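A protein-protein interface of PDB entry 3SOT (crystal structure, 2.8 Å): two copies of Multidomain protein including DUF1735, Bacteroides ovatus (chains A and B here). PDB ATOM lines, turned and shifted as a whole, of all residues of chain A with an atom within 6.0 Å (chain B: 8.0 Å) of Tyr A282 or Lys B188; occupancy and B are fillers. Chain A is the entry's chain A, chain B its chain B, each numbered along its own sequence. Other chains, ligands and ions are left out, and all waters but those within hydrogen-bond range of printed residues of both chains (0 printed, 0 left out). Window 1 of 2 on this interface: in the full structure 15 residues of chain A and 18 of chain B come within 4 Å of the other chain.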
ATOM      1  N   TYR A 218      19.500  22.196  10.586  1.00  0.00           N
ATOM      2  CA  TYR A 218      18.978  23.324   9.828  1.00  0.00           C
ATOM      3  C   TYR A 218      17.647  23.867  10.396  1.00  0.00           C
ATOM      4  O   TYR A 218      16.951  24.617   9.703  1.00  0.00           O
ATOM      5  CB  TYR A 218      18.777  22.933   8.370  1.00  0.00           C
ATOM      6  CG  TYR A 218      20.067  22.531   7.693  1.00  0.00           C
ATOM      7  CD1 TYR A 218      20.958  23.488   7.216  1.00  0.00           C
ATOM      8  CD2 TYR A 218      20.400  21.187   7.529  1.00  0.00           C
ATOM      9  CE1 TYR A 218      22.155  23.117   6.609  1.00  0.00           C
ATOM     10  CE2 TYR A 218      21.603  20.809   6.939  1.00  0.00           C
ATOM     11  CZ  TYR A 218      22.463  21.777   6.465  1.00  0.00           C
ATOM     12  OH  TYR A 218      23.625  21.392   5.858  1.00  0.00           O
ATOM     13  N   ASP A 279      24.611  25.192   3.515  1.00  0.00           N
ATOM     14  CA  ASP A 279      24.315  23.777   3.371  1.00  0.00           C
ATOM     15  C   ASP A 279      25.685  23.080   3.332  1.00  0.00           C
ATOM     16  O   ASP A 279      26.470  23.248   2.375  1.00  0.00           O
ATOM     17  CB  ASP A 279      23.407  23.476   2.140  1.00  0.00           C
ATOM     18  CG  ASP A 279      23.078  22.004   1.886  1.00  0.00           C
ATOM     19  OD1 ASP A 279      23.817  21.138   2.375  1.00  0.00           O
ATOM     20  OD2 ASP A 279      22.106  21.729   1.157  1.00  0.00           O
ATOM     21  N   PHE A 280      25.984  22.363   4.413  1.00  0.00           N
ATOM     22  CA  PHE A 280      27.260  21.677   4.589  1.00  0.00           C
ATOM     23  C   PHE A 280      27.046  20.158   4.623  1.00  0.00           C
ATOM     24  O   PHE A 280      27.955  19.439   5.011  1.00  0.00           O
ATOM     25  CB  PHE A 280      27.928  22.182   5.902  1.00  0.00           C
ATOM     26  CG  PHE A 280      27.136  21.914   7.159  1.00  0.00           C
ATOM     27  CD1 PHE A 280      26.104  22.765   7.543  1.00  0.00           C
ATOM     28  CD2 PHE A 280      27.422  20.817   7.960  1.00  0.00           C
ATOM     29  CE1 PHE A 280      25.352  22.509   8.682  1.00  0.00           C
ATOM     30  CE2 PHE A 280      26.663  20.553   9.092  1.00  0.00           C
ATOM     31  CZ  PHE A 280      25.638  21.409   9.451  1.00  0.00           C
ATOM     32  N   THR A 281      25.847  19.679   4.247  1.00  0.00           N
ATOM     33  CA  THR A 281      25.475  18.257   4.287  1.00  0.00           C
ATOM     34  C   THR A 281      24.912  17.715   2.933  1.00  0.00           C
ATOM     35  O   THR A 281      24.461  16.566   2.893  1.00  0.00           O
ATOM     36  CB  THR A 281      24.404  18.054   5.363  1.00  0.00           C
ATOM     37  OG1 THR A 281      23.274  18.865   5.025  1.00  0.00           O
ATOM     38  CG2 THR A 281      24.894  18.361   6.771  1.00  0.00           C
ATOM     39  N   TYR A 282      24.970  18.518   1.838  1.00  0.00           N
ATOM     40  CA  TYR A 282      24.445  18.175   0.516  1.00  0.00           C
ATOM     41  C   TYR A 282      25.197  17.004  -0.167  1.00  0.00           C
ATOM     42  O   TYR A 282      24.688  16.461  -1.158  1.00  0.00           O
ATOM     43  CB  TYR A 282      24.482  19.394  -0.429  1.00  0.00           C
ATOM     44  CG  TYR A 282      25.855  19.939  -0.721  1.00  0.00           C
ATOM     45  CD1 TYR A 282      26.619  19.440  -1.777  1.00  0.00           C
ATOM     46  CD2 TYR A 282      26.365  21.000   0.001  1.00  0.00           C
ATOM     47  CE1 TYR A 282      27.906  19.913  -2.030  1.00  0.00           C
ATOM     48  CE2 TYR A 282      27.634  21.511  -0.270  1.00  0.00           C
ATOM     49  CZ  TYR A 282      28.406  20.960  -1.282  1.00  0.00           C
ATOM     50  OH  TYR A 282      29.664  21.444  -1.558  1.00  0.00           O
ATOM     51  N   GLY A 283      26.386  16.659   0.321  1.00  0.00           N
ATOM     52  CA  GLY A 283      27.194  15.606  -0.278  1.00  0.00           C
ATOM     53  C   GLY A 283      26.785  14.205   0.117  1.00  0.00           C
ATOM     54  O   GLY A 283      27.232  13.220  -0.482  1.00  0.00           O
ATOM     55  N   GLY A 284      25.906  14.130   1.096  1.00  0.00           N
ATOM     56  CA  GLY A 284      25.495  12.892   1.720  1.00  0.00           C
ATOM     57  C   GLY A 284      26.155  12.908   3.085  1.00  0.00           C
ATOM     58  O   GLY A 284      26.649  13.962   3.531  1.00  0.00           O
ATOM     59  N   VAL A 289      32.314  18.615   2.859  1.00  0.00           N
ATOM     60  CA  VAL A 289      32.139  19.328   1.597  1.00  0.00           C
ATOM     61  C   VAL A 289      32.325  20.849   1.794  1.00  0.00           C
ATOM     62  O   VAL A 289      32.270  21.353   2.913  1.00  0.00           O
ATOM     63  CB  VAL A 289      30.712  19.022   1.001  1.00  0.00           C
ATOM     64  CG1 VAL A 289      30.574  17.582   0.543  1.00  0.00           C
ATOM     65  CG2 VAL A 289      29.588  19.380   1.979  1.00  0.00           C
ATOM     66  N   ILE A 290      32.507  21.572   0.684  1.00  0.00           N
ATOM     67  CA  ILE A 290      32.567  23.030   0.677  1.00  0.00           C
ATOM     68  C   ILE A 290      31.153  23.530   0.938  1.00  0.00           C
ATOM     69  O   ILE A 290      30.257  23.216   0.153  1.00  0.00           O
ATOM     70  CB  ILE A 290      33.169  23.580  -0.645  1.00  0.00           C
ATOM     71  CG1 ILE A 290      34.555  22.930  -0.948  1.00  0.00           C
ATOM     72  CG2 ILE A 290      33.214  25.102  -0.632  1.00  0.00           C
ATOM     73  CD1 ILE A 290      35.138  23.221  -2.229  1.00  0.00           C
ATOM     74  N   PRO A 291      30.881  24.261   2.052  1.00  0.00           N
ATOM     75  CA  PRO A 291      29.521  24.720   2.284  1.00  0.00           C
ATOM     76  C   PRO A 291      29.083  25.685   1.191  1.00  0.00           C
ATOM     77  O   PRO A 291      29.904  26.436   0.654  1.00  0.00           O
ATOM     78  CB  PRO A 291      29.625  25.395   3.645  1.00  0.00           C
ATOM     79  CG  PRO A 291      30.817  24.809   4.280  1.00  0.00           C
ATOM     80  CD  PRO A 291      31.760  24.716   3.151  1.00  0.00           C
ATOM     81  N   ILE A 292      27.792  25.584   0.811  1.00  0.00           N
ATOM     82  CA  ILE A 292      27.136  26.438  -0.186  1.00  0.00           C
ATOM     83  C   ILE A 292      26.347  27.450   0.601  1.00  0.00           C
ATOM     84  O   ILE A 292      25.372  27.096   1.282  1.00  0.00           O
ATOM     85  CB  ILE A 292      26.278  25.657  -1.225  1.00  0.00           C
ATOM     86  CG1 ILE A 292      27.128  24.636  -1.998  1.00  0.00           C
ATOM     87  CG2 ILE A 292      25.601  26.613  -2.194  1.00  0.00           C
ATOM     88  CD1 ILE A 292      26.301  23.645  -2.837  1.00  0.00           C
ATOM     89  N   GLY B 162      36.007  12.734  -7.177  1.00  0.00           N
ATOM     90  CA  GLY B 162      35.094  12.883  -6.056  1.00  0.00           C
ATOM     91  C   GLY B 162      33.897  13.739  -6.396  1.00  0.00           C
ATOM     92  O   GLY B 162      33.567  13.949  -7.569  1.00  0.00           O
ATOM     93  N   SER B 163      33.246  14.244  -5.355  1.00  0.00           N
ATOM     94  CA  SER B 163      32.063  15.067  -5.458  1.00  0.00           C
ATOM     95  C   SER B 163      32.477  16.530  -5.453  1.00  0.00           C
ATOM     96  O   SER B 163      32.919  17.065  -4.422  1.00  0.00           O
ATOM     97  CB  SER B 163      31.109  14.736  -4.317  1.00  0.00           C
ATOM     98  OG  SER B 163      29.897  15.467  -4.383  1.00  0.00           O
ATOM     99  N   TYR B 164      32.403  17.157  -6.646  1.00  0.00           N
ATOM    100  CA  TYR B 164      32.693  18.574  -6.893  1.00  0.00           C
ATOM    101  C   TYR B 164      31.511  19.431  -6.559  1.00  0.00           C
ATOM    102  O   TYR B 164      30.403  19.050  -6.916  1.00  0.00           O
ATOM    103  CB  TYR B 164      33.061  18.788  -8.373  1.00  0.00           C
ATOM    104  CG  TYR B 164      34.487  18.456  -8.767  1.00  0.00           C
ATOM    105  CD1 TYR B 164      34.884  17.141  -8.971  1.00  0.00           C
ATOM    106  CD2 TYR B 164      35.395  19.464  -9.074  1.00  0.00           C
ATOM    107  CE1 TYR B 164      36.186  16.834  -9.358  1.00  0.00           C
ATOM    108  CE2 TYR B 164      36.689  19.171  -9.485  1.00  0.00           C
ATOM    109  CZ  TYR B 164      37.085  17.854  -9.613  1.00  0.00           C
ATOM    110  OH  TYR B 164      38.367  17.579 -10.007  1.00  0.00           O
ATOM    111  N   THR B 165      31.723  20.598  -5.914  1.00  0.00           N
ATOM    112  CA  THR B 165      30.679  21.592  -5.620  1.00  0.00           C
ATOM    113  C   THR B 165      30.374  22.246  -6.947  1.00  0.00           C
ATOM    114  O   THR B 165      31.302  22.737  -7.566  1.00  0.00           O
ATOM    115  CB  THR B 165      31.155  22.566  -4.505  1.00  0.00           C
ATOM    116  OG1 THR B 165      31.479  21.818  -3.335  1.00  0.00           O
ATOM    117  CG2 THR B 165      30.123  23.646  -4.160  1.00  0.00           C
ATOM    118  N   ALA B 166      29.124  22.219  -7.422  1.00  0.00           N
ATOM    119  CA  ALA B 166      28.813  22.755  -8.748  1.00  0.00           C
ATOM    120  C   ALA B 166      27.861  23.960  -8.690  1.00  0.00           C
ATOM    121  O   ALA B 166      27.191  24.254  -9.684  1.00  0.00           O
ATOM    122  CB  ALA B 166      28.192  21.650  -9.602  1.00  0.00           C
ATOM    123  N   SER B 167      27.829  24.683  -7.558  1.00  0.00           N
ATOM    124  CA  SER B 167      26.921  25.832  -7.332  1.00  0.00           C
ATOM    125  C   SER B 167      27.272  27.056  -8.234  1.00  0.00           C
ATOM    126  O   SER B 167      26.393  27.893  -8.482  1.00  0.00           O
ATOM    127  CB  SER B 167      26.950  26.256  -5.866  1.00  0.00           C
ATOM    128  OG  SER B 167      28.249  26.614  -5.433  1.00  0.00           O
ATOM    129  N   MET B 169      28.490  26.557 -11.366  1.00  0.00           N
ATOM    130  CA  MET B 169      28.287  26.027 -12.720  1.00  0.00           C
ATOM    131  C   MET B 169      26.858  26.341 -13.204  1.00  0.00           C
ATOM    132  O   MET B 169      25.882  25.807 -12.655  1.00  0.00           O
ATOM    133  CB  MET B 169      28.550  24.530 -12.813  1.00  0.00           C
ATOM    134  CG  MET B 169      28.370  24.030 -14.234  1.00  0.00           C
ATOM    135  SD  MET B 169      28.415  22.132 -14.530  1.00  0.00           S
ATOM    136  CE  MET B 169      26.831  21.628 -13.549  1.00  0.00           C
ATOM    137  N   THR B 185      21.137  25.483 -12.081  1.00  0.00           N
ATOM    138  CA  THR B 185      22.302  25.002 -11.337  1.00  0.00           C
ATOM    139  C   THR B 185      21.926  23.811 -10.487  1.00  0.00           C
ATOM    140  O   THR B 185      20.752  23.575 -10.266  1.00  0.00           O
ATOM    141  CB  THR B 185      22.893  26.131 -10.435  1.00  0.00           C
ATOM    142  OG1 THR B 185      21.930  26.539  -9.459  1.00  0.00           O
ATOM    143  CG2 THR B 185      23.429  27.327 -11.215  1.00  0.00           C
ATOM    144  N   THR B 186      22.926  23.065 -10.010  1.00  0.00           N
ATOM    145  CA  THR B 186      22.776  21.959  -9.059  1.00  0.00           C
ATOM    146  C   THR B 186      23.843  22.194  -7.995  1.00  0.00           C
ATOM    147  O   THR B 186      24.710  23.051  -8.204  1.00  0.00           O
ATOM    148  CB  THR B 186      22.825  20.565  -9.706  1.00  0.00           C
ATOM    149  OG1 THR B 186      22.432  19.639  -8.702  1.00  0.00           O
ATOM    150  CG2 THR B 186      24.207  20.195 -10.283  1.00  0.00           C
ATOM    151  N   ASP B 187      23.797  21.457  -6.879  1.00  0.00           N
ATOM    152  CA  ASP B 187      24.728  21.671  -5.772  1.00  0.00           C
ATOM    153  C   ASP B 187      26.059  20.898  -5.966  1.00  0.00           C
ATOM    154  O   ASP B 187      27.094  21.376  -5.489  1.00  0.00           O
ATOM    155  CB  ASP B 187      24.090  21.283  -4.429  1.00  0.00           C
ATOM    156  CG  ASP B 187      23.394  19.944  -4.354  1.00  0.00           C
ATOM    157  OD1 ASP B 187      23.497  19.148  -5.338  1.00  0.00           O
ATOM    158  OD2 ASP B 187      22.697  19.704  -3.339  1.00  0.00           O
ATOM    159  N   LYS B 188      26.038  19.733  -6.666  1.00  0.00           N
ATOM    160  CA  LYS B 188      27.232  18.913  -6.868  1.00  0.00           C
ATOM    161  C   LYS B 188      27.150  18.023  -8.128  1.00  0.00           C
ATOM    162  O   LYS B 188      26.051  17.657  -8.557  1.00  0.00           O
ATOM    163  CB  LYS B 188      27.442  18.017  -5.650  1.00  0.00           C
ATOM    164  CG  LYS B 188      26.299  17.037  -5.447  1.00  0.00           C
ATOM    165  CD  LYS B 188      26.441  16.094  -4.290  1.00  0.00           C
ATOM    166  CE  LYS B 188      25.161  15.296  -4.267  1.00  0.00           C
ATOM    167  NZ  LYS B 188      25.162  14.255  -3.229  1.00  0.00           N
ATOM    168  N   ARG B 189      28.328  17.654  -8.689  1.00  0.00           N
ATOM    169  CA  ARG B 189      28.546  16.739  -9.820  1.00  0.00           C
ATOM    170  C   ARG B 189      29.686  15.848  -9.453  1.00  0.00           C
ATOM    171  O   ARG B 189      30.638  16.323  -8.831  1.00  0.00           O
ATOM    172  CB  ARG B 189      28.813  17.474 -11.162  1.00  0.00           C
ATOM    173  CG  ARG B 189      27.703  18.403 -11.686  1.00  0.00           C
ATOM    174  CD  ARG B 189      26.427  17.685 -12.091  1.00  0.00           C
ATOM    175  NE  ARG B 189      26.533  16.937 -13.346  1.00  0.00           N
ATOM    176  CZ  ARG B 189      25.585  16.115 -13.782  1.00  0.00           C
ATOM    177  NH1 ARG B 189      24.510  15.888 -13.043  1.00  0.00           N
ATOM    178  NH2 ARG B 189      25.721  15.485 -14.936  1.00  0.00           N
ATOM    179  N   THR B 190      29.641  14.566  -9.864  1.00  0.00           N
ATOM    180  CA  THR B 190      30.677  13.578  -9.545  1.00  0.00           C
ATOM    181  C   THR B 190      31.657  13.475 -10.681  1.00  0.00           C
ATOM    182  O   THR B 190      31.262  13.355 -11.835  1.00  0.00           O
ATOM    183  CB  THR B 190      30.025  12.211  -9.247  1.00  0.00           C
ATOM    184  OG1 THR B 190      28.957  12.386  -8.302  1.00  0.00           O
ATOM    185  CG2 THR B 190      31.011  11.196  -8.711  1.00  0.00           C
ATOM    186  N   GLY B 191      32.938  13.472 -10.328  1.00  0.00           N
ATOM    187  CA  GLY B 191      34.076  13.302 -11.231  1.00  0.00           C
ATOM    188  C   GLY B 191      34.572  11.901 -11.000  1.00  0.00           C
ATOM    189  O   GLY B 191      35.010  11.563  -9.899  1.00  0.00           O
ATOM    190  N   PHE B 201      33.044  13.397 -16.300  1.00  0.00           N
ATOM    191  CA  PHE B 201      31.789  13.953 -15.810  1.00  0.00           C
ATOM    192  C   PHE B 201      30.681  13.658 -16.777  1.00  0.00           C
ATOM    193  O   PHE B 201      30.965  13.391 -17.939  1.00  0.00           O
ATOM    194  CB  PHE B 201      31.872  15.488 -15.595  1.00  0.00           C
ATOM    195  CG  PHE B 201      32.778  16.012 -14.522  1.00  0.00           C
ATOM    196  CD1 PHE B 201      32.312  16.193 -13.221  1.00  0.00           C
ATOM    197  CD2 PHE B 201      34.075  16.421 -14.824  1.00  0.00           C
ATOM    198  CE1 PHE B 201      33.151  16.707 -12.229  1.00  0.00           C
ATOM    199  CE2 PHE B 201      34.907  16.947 -13.827  1.00  0.00           C
ATOM    200  CZ  PHE B 201      34.435  17.086 -12.541  1.00  0.00           C
ATOM    201  N   GLY B 204      26.643  18.836 -18.461  1.00  0.00           N
ATOM    202  CA  GLY B 204      25.639  19.707 -17.863  1.00  0.00           C
ATOM    203  C   GLY B 204      25.006  19.151 -16.612  1.00  0.00           C
ATOM    204  O   GLY B 204      25.712  18.822 -15.649  1.00  0.00           O
ATOM    205  N   LEU B 205      23.660  19.008 -16.646  1.00  0.00           N
ATOM    206  CA  LEU B 205      22.863  18.519 -15.523  1.00  0.00           C
ATOM    207  C   LEU B 205      22.245  17.160 -15.829  1.00  0.00           C
ATOM    208  O   LEU B 205      21.303  16.757 -15.132  1.00  0.00           O
ATOM    209  CB  LEU B 205      21.756  19.539 -15.173  1.00  0.00           C
ATOM    210  CG  LEU B 205      22.221  20.963 -14.795  1.00  0.00           C
ATOM    211  CD1 LEU B 205      21.055  21.875 -14.612  1.00  0.00           C
ATOM    212  CD2 LEU B 205      23.101  20.966 -13.539  1.00  0.00           C
ATOM    213  N   ILE B 206      22.814  16.421 -16.806  1.00  0.00           N
ATOM    214  CA  ILE B 206      22.371  15.075 -17.182  1.00  0.00           C
ATOM    215  C   ILE B 206      22.322  14.226 -15.910  1.00  0.00           C
ATOM    216  O   ILE B 206      23.272  14.257 -15.100  1.00  0.00           O
ATOM    217  CB  ILE B 206      23.311  14.472 -18.293  1.00  0.00           C
ATOM    218  CG1 ILE B 206      23.038  15.109 -19.676  1.00  0.00           C
ATOM    219  CG2 ILE B 206      23.294  12.949 -18.382  1.00  0.00           C
ATOM    220  CD1 ILE B 206      21.623  14.942 -20.290  1.00  0.00           C
ATOM    221  N   GLU B 208      22.885  11.512 -13.491  1.00  0.00           N
ATOM    222  CA  GLU B 208      23.945  10.524 -13.251  1.00  0.00           C
ATOM    223  C   GLU B 208      23.377   9.116 -12.994  1.00  0.00           C
ATOM    224  O   GLU B 208      24.158   8.158 -12.996  1.00  0.00           O
ATOM    225  CB  GLU B 208      24.821  10.940 -12.044  1.00  0.00           C
ATOM    226  CG  GLU B 208      25.590  12.244 -12.244  1.00  0.00           C
ATOM    227  CD  GLU B 208      26.492  12.718 -11.110  1.00  0.00           C
ATOM    228  OE1 GLU B 208      26.355  12.207  -9.976  1.00  0.00           O
ATOM    229  OE2 GLU B 208      27.326  13.622 -11.357  1.00  0.00           O
ATOM    230  N   MET B 300      33.717  24.443 -10.888  1.00  0.00           N
ATOM    231  CA  MET B 300      33.417  23.406  -9.911  1.00  0.00           C
ATOM    232  C   MET B 300      34.633  23.219  -9.058  1.00  0.00           C
ATOM    233  O   MET B 300      35.735  23.367  -9.578  1.00  0.00           O
ATOM    234  CB  MET B 300      32.979  22.108 -10.558  1.00  0.00           C
ATOM    235  CG  MET B 300      31.623  22.191 -11.226  1.00  0.00           C
ATOM    236  SD  MET B 300      31.040  20.437 -11.693  1.00  0.00           S
ATOM    237  CE  MET B 300      32.143  20.073 -13.187  1.00  0.00           C
ATOM    238  N   THR B 301      34.461  22.967  -7.740  1.00  0.00           N
ATOM    239  CA  THR B 301      35.604  22.834  -6.845  1.00  0.00           C
ATOM    240  C   THR B 301      35.477  21.572  -6.027  1.00  0.00           C
ATOM    241  O   THR B 301      34.437  21.317  -5.429  1.00  0.00           O
ATOM    242  CB  THR B 301      35.734  24.067  -5.943  1.00  0.00           C
ATOM    243  OG1 THR B 301      35.682  25.253  -6.752  1.00  0.00           O
ATOM    244  CG2 THR B 301      37.025  24.060  -5.123  1.00  0.00           C
ATOM    245  N   LEU B 303      36.871  19.382  -2.774  1.00  0.00           N
ATOM    246  CA  LEU B 303      37.569  19.459  -1.480  1.00  0.00           C
ATOM    247  C   LEU B 303      38.058  18.064  -1.065  1.00  0.00           C
ATOM    248  O   LEU B 303      37.369  17.067  -1.257  1.00  0.00           O
ATOM    249  CB  LEU B 303      36.669  20.067  -0.405  1.00  0.00           C
ATOM    250  CG  LEU B 303      37.127  20.081   1.049  1.00  0.00           C
ATOM    251  CD1 LEU B 303      38.348  20.909   1.244  1.00  0.00           C
ATOM    252  CD2 LEU B 303      36.039  20.561   1.940  1.00  0.00           C
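Of chain B, only Thr B165 (2.6 Å), Asp B187 (3.4 Å) and Lys B188 (3.1 Å) come within 4 Å of Tyr A282. Gly A283 touches one residue of chain B. Of the printed residues of chain B, Ile A290 touches Thr B165, Thr B301 and Leu B303. Printed residues of chain A within 4 Å of Ser B167: Ile A292. Lys B188 touches two residues of chain A. Of the printed residues of chain A, Thr B301 touches Ile A290 (3.6 Å). Printed residues of chain A within 4 Å of Leu B303: Val A289 (3.7 Å) and Ile A290 (3.6 Å). The nearest residue of chain A that does not touch Lys B188 is Gly A284 (4.4 Å). The nearest printed residue of chain B that does not touch Val A289 is Thr B165 (5.2 Å).
The side-chain carboxylate of Asp A279 is in hydrogen-bond range of the backbone NH of Tyr A282. N of Asp A279 lies within hydrogen-bond range of O of Ile A292 (3.0 Å). O of Ile A290 sits at hydrogen-bond distance from OH of Tyr A282, 2.5 Å away. N of Thr B165 sits at hydrogen-bond distance from O of Thr B301 (2.8 Å). The backbone NH (N) of Ala B166 is in hydrogen-bond range of the backbone carbonyl oxygen (O) of Asp B187 (2.9 Å).
No position is printed for both chains.
Hydrophobic or aromatic side chains of chain A that line the printed part of chain B: Tyr A282, Ile A290 and Ile A292. Of the 22 printed residues of chain B, 6 touch a printed residue of chain A. Hydrophobic or aromatic side chains of chain B that line the printed part of chain A: Leu B303. Along chain B the printed residues that touch a printed residue of chain A span positions 165 to 303. Among the printed residues, no Asp or Glu carboxylate lies within 4 Å of a Lys or Arg side-chain nitrogen of the other chain.
OG1 of Thr B165 is in hydrogen-bond range of OH of Tyr A282 (2.6 Å). NZ of Lys B188 sits at hydrogen-bond distance from O of Tyr A282 (3.1 Å).
Among the printed residues, pairs that only touch across the chains: Tyr A282 with Asp B187, Ile A290 with Thr B301, Ile A292 with Asp B187, Gly A283 with Lys B188, Ile A290 with Leu B303, Ile A290 with Thr B165, Val A289 with Leu B303, Ile A292 with Thr B165 and Ile A292 with Ser B167.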
